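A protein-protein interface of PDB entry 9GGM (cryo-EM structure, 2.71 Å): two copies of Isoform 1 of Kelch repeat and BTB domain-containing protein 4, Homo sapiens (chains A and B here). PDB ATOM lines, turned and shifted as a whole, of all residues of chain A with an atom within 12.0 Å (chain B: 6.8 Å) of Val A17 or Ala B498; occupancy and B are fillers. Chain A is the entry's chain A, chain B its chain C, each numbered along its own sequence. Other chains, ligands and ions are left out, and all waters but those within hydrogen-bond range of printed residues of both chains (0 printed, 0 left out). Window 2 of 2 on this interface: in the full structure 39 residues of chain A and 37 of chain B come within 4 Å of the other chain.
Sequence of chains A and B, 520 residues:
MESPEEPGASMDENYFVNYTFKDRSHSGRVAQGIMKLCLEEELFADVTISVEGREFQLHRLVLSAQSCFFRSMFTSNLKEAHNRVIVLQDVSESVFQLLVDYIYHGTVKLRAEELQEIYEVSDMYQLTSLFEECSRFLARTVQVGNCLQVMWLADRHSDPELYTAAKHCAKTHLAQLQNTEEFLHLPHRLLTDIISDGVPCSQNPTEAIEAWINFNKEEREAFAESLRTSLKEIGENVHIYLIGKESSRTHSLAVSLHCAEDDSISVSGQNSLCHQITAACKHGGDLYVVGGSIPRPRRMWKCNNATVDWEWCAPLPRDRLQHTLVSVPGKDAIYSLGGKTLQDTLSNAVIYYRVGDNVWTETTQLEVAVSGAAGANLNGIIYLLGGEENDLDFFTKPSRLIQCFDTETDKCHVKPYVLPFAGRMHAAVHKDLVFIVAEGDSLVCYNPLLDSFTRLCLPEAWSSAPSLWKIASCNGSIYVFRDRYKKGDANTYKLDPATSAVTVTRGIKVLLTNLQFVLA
Phe A16 touches Phe B137. Phe A16 touches Pro B497. Arg B111 touches Val A17 (CA to O, 3.6 Å). Ala B498 touches Val A17. Leu B110 touches Asn A18 (O to CA, 3.8 Å). Asn A18 touches Thr B454. Lys B109 touches Tyr A19 (CA to O, 3.5 Å). Leu B110 touches Tyr A19. Tyr A19 touches Phe B137.
No position is printed for both chains. Of the 10 pairs that touch across the chains among the printed residues, none has its exchanged pair printed and touching as well.
The backbone carbonyl oxygen (O) of Val A17 sits close to the backbone carbonyl oxygen (O) of Leu B110 (2.7 Å).
Hydrophobic or aromatic side chains of chain B within 4 Å of the printed part of chain A: Leu B110, Phe B137 and Pro B497. Among the printed residues, 10 pairs touch across the chains.
Of chain B, only Leu B110 (2.7 Å), Arg B111 (3.6 Å) and Ala B498 (3.5 Å) come within 4 Å of Val A17. Of chain A, only Val A17 (3.5 Å) comes within 4 Å of Ala B498. Of the printed residues of chain A, Lys B109 touches Tyr A19 (3.5 Å). Printed residues of chain B within 4 Å of Phe A16: Phe B137 and Pro B497. Leu B495 touches none of the printed residues of chain A. The nearest residue of chain B that does not touch Val A17 is Ala B112 (4.1 Å).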
ATOM      1  N   PHE A  16      16.853   5.130 -23.611  1.00  0.00           N
ATOM      2  CA  PHE A  16      17.635   4.205 -22.800  1.00  0.00           C
ATOM      3  C   PHE A  16      18.531   4.924 -21.798  1.00  0.00           C
ATOM      4  O   PHE A  16      19.075   4.300 -20.887  1.00  0.00           O
ATOM      5  CB  PHE A  16      18.471   3.289 -23.694  1.00  0.00           C
ATOM      6  CG  PHE A  16      17.732   2.070 -24.166  1.00  0.00           C
ATOM      7  CD1 PHE A  16      16.891   2.130 -25.263  1.00  0.00           C
ATOM      8  CD2 PHE A  16      17.885   0.860 -23.510  1.00  0.00           C
ATOM      9  CE1 PHE A  16      16.212   1.004 -25.692  1.00  0.00           C
ATOM     10  CE2 PHE A  16      17.210  -0.267 -23.935  1.00  0.00           C
ATOM     11  CZ  PHE A  16      16.374  -0.195 -25.028  1.00  0.00           C
ATOM     12  N   VAL A  17      18.684   6.239 -21.962  1.00  0.00           N
ATOM     13  CA  VAL A  17      19.533   7.036 -21.090  1.00  0.00           C
ATOM     14  C   VAL A  17      18.766   8.171 -20.424  1.00  0.00           C
ATOM     15  O   VAL A  17      18.919   8.399 -19.220  1.00  0.00           O
ATOM     16  CB  VAL A  17      20.757   7.587 -21.857  1.00  0.00           C
ATOM     17  CG1 VAL A  17      21.848   6.532 -21.939  1.00  0.00           C
ATOM     18  CG2 VAL A  17      20.352   8.043 -23.249  1.00  0.00           C
ATOM     19  N   ASN A  18      17.947   8.903 -21.179  1.00  0.00           N
ATOM     20  CA  ASN A  18      17.259  10.063 -20.629  1.00  0.00           C
ATOM     21  C   ASN A  18      15.883  10.224 -21.256  1.00  0.00           C
ATOM     22  O   ASN A  18      15.751  10.118 -22.477  1.00  0.00           O
ATOM     23  CB  ASN A  18      18.089  11.334 -20.849  1.00  0.00           C
ATOM     24  CG  ASN A  18      17.244  12.593 -20.833  1.00  0.00           C
ATOM     25  OD1 ASN A  18      16.824  13.060 -19.775  1.00  0.00           O
ATOM     26  ND2 ASN A  18      16.994  13.151 -22.011  1.00  0.00           N
ATOM     27  N   TYR A  19      14.866  10.452 -20.422  1.00  0.00           N
ATOM     28  CA  TYR A  19      13.501  10.714 -20.871  1.00  0.00           C
ATOM     29  C   TYR A  19      12.771  11.295 -19.669  1.00  0.00           C
ATOM     30  O   TYR A  19      13.127  11.007 -18.523  1.00  0.00           O
ATOM     31  CB  TYR A  19      12.718   9.502 -21.391  1.00  0.00           C
ATOM     32  CG  TYR A  19      12.431   8.436 -20.373  1.00  0.00           C
ATOM     33  CD1 TYR A  19      13.439   7.815 -19.671  1.00  0.00           C
ATOM     34  CD2 TYR A  19      11.117   8.088 -20.084  1.00  0.00           C
ATOM     35  CE1 TYR A  19      13.151   6.862 -18.734  1.00  0.00           C
ATOM     36  CE2 TYR A  19      10.821   7.130 -19.145  1.00  0.00           C
ATOM     37  CZ  TYR A  19      11.846   6.518 -18.468  1.00  0.00           C
ATOM     38  OH  TYR A  19      11.569   5.552 -17.527  1.00  0.00           O
ATOM     39  N   THR A  20      11.751  12.104 -19.927  1.00  0.00           N
ATOM     40  CA  THR A  20      10.911  12.627 -18.857  1.00  0.00           C
ATOM     41  C   THR A  20       9.651  11.778 -18.727  1.00  0.00           C
ATOM     42  O   THR A  20       8.984  11.484 -19.724  1.00  0.00           O
ATOM     43  CB  THR A  20      10.535  14.086 -19.119  1.00  0.00           C
ATOM     44  N   PHE A  21       9.341  11.387 -17.487  1.00  0.00           N
ATOM     45  CA  PHE A  21       8.178  10.568 -17.145  1.00  0.00           C
ATOM     46  C   PHE A  21       7.140  11.451 -16.461  1.00  0.00           C
ATOM     47  O   PHE A  21       7.348  11.914 -15.334  1.00  0.00           O
ATOM     48  CB  PHE A  21       8.614   9.392 -16.262  1.00  0.00           C
ATOM     49  CG  PHE A  21       7.489   8.686 -15.533  1.00  0.00           C
ATOM     50  CD1 PHE A  21       6.271   8.434 -16.135  1.00  0.00           C
ATOM     51  CD2 PHE A  21       7.686   8.229 -14.241  1.00  0.00           C
ATOM     52  CE1 PHE A  21       5.264   7.773 -15.455  1.00  0.00           C
ATOM     53  CE2 PHE A  21       6.688   7.568 -13.560  1.00  0.00           C
ATOM     54  CZ  PHE A  21       5.474   7.340 -14.166  1.00  0.00           C
ATOM     55  N   LYS B 109      12.851  11.671 -14.086  1.00  0.00           N
ATOM     56  CA  LYS B 109      13.795  11.365 -15.147  1.00  0.00           C
ATOM     57  C   LYS B 109      14.857  10.421 -14.605  1.00  0.00           C
ATOM     58  O   LYS B 109      15.235  10.495 -13.431  1.00  0.00           O
ATOM     59  CB  LYS B 109      14.450  12.636 -15.699  1.00  0.00           C
ATOM     60  N   LEU B 110      15.333   9.526 -15.466  1.00  0.00           N
ATOM     61  CA  LEU B 110      16.326   8.532 -15.091  1.00  0.00           C
ATOM     62  C   LEU B 110      17.630   8.735 -15.845  1.00  0.00           C
ATOM     63  O   LEU B 110      17.654   9.237 -16.973  1.00  0.00           O
ATOM     64  CB  LEU B 110      15.854   7.080 -15.298  1.00  0.00           C
ATOM     65  CG  LEU B 110      15.825   6.403 -16.668  1.00  0.00           C
ATOM     66  CD1 LEU B 110      17.159   5.819 -17.092  1.00  0.00           C
ATOM     67  CD2 LEU B 110      14.843   5.258 -16.523  1.00  0.00           C
ATOM     68  N   ARG B 111      18.709   8.348 -15.183  1.00  0.00           N
ATOM     69  CA  ARG B 111      20.002   8.099 -15.797  1.00  0.00           C
ATOM     70  C   ARG B 111      20.300   6.611 -15.669  1.00  0.00           C
ATOM     71  O   ARG B 111      19.848   5.954 -14.729  1.00  0.00           O
ATOM     72  CB  ARG B 111      21.099   8.938 -15.137  1.00  0.00           C
ATOM     73  CG  ARG B 111      21.438  10.220 -15.886  1.00  0.00           C
ATOM     74  CD  ARG B 111      20.206  11.087 -16.107  1.00  0.00           C
ATOM     75  NE  ARG B 111      19.587  11.513 -14.858  1.00  0.00           N
ATOM     76  CZ  ARG B 111      18.581  12.373 -14.778  1.00  0.00           C
ATOM     77  NH1 ARG B 111      18.050  12.919 -15.860  1.00  0.00           N
ATOM     78  NH2 ARG B 111      18.093  12.692 -13.583  1.00  0.00           N
ATOM     79  N   ALA B 112      21.025   6.071 -16.650  1.00  0.00           N
ATOM     80  CA  ALA B 112      21.080   4.621 -16.835  1.00  0.00           C
ATOM     81  C   ALA B 112      21.559   3.880 -15.588  1.00  0.00           C
ATOM     82  O   ALA B 112      21.216   2.708 -15.399  1.00  0.00           O
ATOM     83  CB  ALA B 112      21.981   4.283 -18.023  1.00  0.00           C
ATOM     84  N   PHE B 137      11.244  -0.479 -18.370  1.00  0.00           N
ATOM     85  CA  PHE B 137      12.479   0.106 -18.880  1.00  0.00           C
ATOM     86  C   PHE B 137      13.647  -0.861 -18.750  1.00  0.00           C
ATOM     87  O   PHE B 137      14.488  -0.950 -19.653  1.00  0.00           O
ATOM     88  CB  PHE B 137      12.770   1.415 -18.145  1.00  0.00           C
ATOM     89  CG  PHE B 137      13.662   2.348 -18.905  1.00  0.00           C
ATOM     90  CD1 PHE B 137      13.127   3.217 -19.840  1.00  0.00           C
ATOM     91  CD2 PHE B 137      15.026   2.368 -18.683  1.00  0.00           C
ATOM     92  CE1 PHE B 137      13.935   4.082 -20.545  1.00  0.00           C
ATOM     93  CE2 PHE B 137      15.842   3.235 -19.385  1.00  0.00           C
ATOM     94  CZ  PHE B 137      15.293   4.094 -20.315  1.00  0.00           C
ATOM     95  N   THR B 454      12.695  11.549 -27.174  1.00  0.00           N
ATOM     96  CA  THR B 454      14.111  11.882 -27.148  1.00  0.00           C
ATOM     97  C   THR B 454      14.725  11.761 -28.537  1.00  0.00           C
ATOM     98  O   THR B 454      14.161  11.136 -29.434  1.00  0.00           O
ATOM     99  CB  THR B 454      14.847  10.988 -26.157  1.00  0.00           C
ATOM    100  OG1 THR B 454      14.758   9.626 -26.585  1.00  0.00           O
ATOM    101  CG2 THR B 454      14.181  11.112 -24.812  1.00  0.00           C
ATOM    102  N   LEU B 456      18.540  11.022 -30.689  1.00  0.00           N
ATOM    103  CA  LEU B 456      19.904  10.512 -30.692  1.00  0.00           C
ATOM    104  C   LEU B 456      20.603  10.943 -31.973  1.00  0.00           C
ATOM    105  O   LEU B 456      20.009  10.904 -33.058  1.00  0.00           O
ATOM    106  CB  LEU B 456      19.944   8.979 -30.571  1.00  0.00           C
ATOM    107  CG  LEU B 456      19.043   8.236 -29.579  1.00  0.00           C
ATOM    108  CD1 LEU B 456      19.575   6.828 -29.375  1.00  0.00           C
ATOM    109  CD2 LEU B 456      18.963   8.957 -28.243  1.00  0.00           C
ATOM    110  N   LEU B 495      23.203   0.167 -33.867  1.00  0.00           N
ATOM    111  CA  LEU B 495      23.000   1.305 -32.983  1.00  0.00           C
ATOM    112  C   LEU B 495      23.035   0.818 -31.540  1.00  0.00           C
ATOM    113  O   LEU B 495      22.246  -0.051 -31.156  1.00  0.00           O
ATOM    114  CB  LEU B 495      21.671   1.993 -33.294  1.00  0.00           C
ATOM    115  CG  LEU B 495      21.372   3.436 -32.867  1.00  0.00           C
ATOM    116  CD1 LEU B 495      19.966   3.797 -33.302  1.00  0.00           C
ATOM    117  CD2 LEU B 495      21.527   3.679 -31.369  1.00  0.00           C
ATOM    118  N   ASP B 496      23.946   1.378 -30.746  1.00  0.00           N
ATOM    119  CA  ASP B 496      24.005   1.076 -29.323  1.00  0.00           C
ATOM    120  C   ASP B 496      23.141   2.095 -28.595  1.00  0.00           C
ATOM    121  O   ASP B 496      23.484   3.286 -28.590  1.00  0.00           O
ATOM    122  CB  ASP B 496      25.437   1.126 -28.815  1.00  0.00           C
ATOM    123  CG  ASP B 496      25.553   0.726 -27.358  1.00  0.00           C
ATOM    124  OD1 ASP B 496      24.765  -0.136 -26.914  1.00  0.00           O
ATOM    125  OD2 ASP B 496      26.433   1.269 -26.659  1.00  0.00           O
ATOM    126  N   PRO B 497      22.025   1.693 -27.980  1.00  0.00           N
ATOM    127  CA  PRO B 497      21.154   2.689 -27.331  1.00  0.00           C
ATOM    128  C   PRO B 497      21.838   3.474 -26.224  1.00  0.00           C
ATOM    129  O   PRO B 497      21.570   4.670 -26.063  1.00  0.00           O
ATOM    130  CB  PRO B 497      19.995   1.838 -26.791  1.00  0.00           C
ATOM    131  CG  PRO B 497      20.073   0.537 -27.535  1.00  0.00           C
ATOM    132  CD  PRO B 497      21.518   0.321 -27.827  1.00  0.00           C
ATOM    133  N   ALA B 498      22.714   2.830 -25.450  1.00  0.00           N
ATOM    134  CA  ALA B 498      23.328   3.498 -24.308  1.00  0.00           C
ATOM    135  C   ALA B 498      24.312   4.574 -24.753  1.00  0.00           C
ATOM    136  O   ALA B 498      24.274   5.708 -24.259  1.00  0.00           O
ATOM    137  CB  ALA B 498      24.021   2.471 -23.413  1.00  0.00           C
ATOM    138  N   THR B 499      25.200   4.239 -25.688  1.00  0.00           N
ATOM    139  CA  THR B 499      26.241   5.148 -26.147  1.00  0.00           C
ATOM    140  C   THR B 499      25.891   5.893 -27.429  1.00  0.00           C
ATOM    141  O   THR B 499      26.629   6.808 -27.807  1.00  0.00           O
ATOM    142  CB  THR B 499      27.555   4.385 -26.357  1.00  0.00           C
ATOM    143  N   SER B 500      24.800   5.526 -28.105  1.00  0.00           N
ATOM    144  CA  SER B 500      24.399   6.131 -29.377  1.00  0.00           C
ATOM    145  C   SER B 500      25.484   6.010 -30.444  1.00  0.00           C
ATOM    146  O   SER B 500      25.509   6.792 -31.399  1.00  0.00           O
ATOM    147  CB  SER B 500      23.995   7.599 -29.196  1.00  0.00           C
ATOM    148  OG  SER B 500      23.405   8.113 -30.378  1.00  0.00           O
ATOM    149  N   ALA B 501      26.382   5.041 -30.297  1.00  0.00           N
ATOM    150  CA  ALA B 501      27.507   4.869 -31.207  1.00  0.00           C
ATOM    151  C   ALA B 501      27.106   3.934 -32.343  1.00  0.00           C
ATOM    152  O   ALA B 501      26.749   2.774 -32.106  1.00  0.00           O
ATOM    153  CB  ALA B 501      28.725   4.322 -30.465  1.00  0.00           C
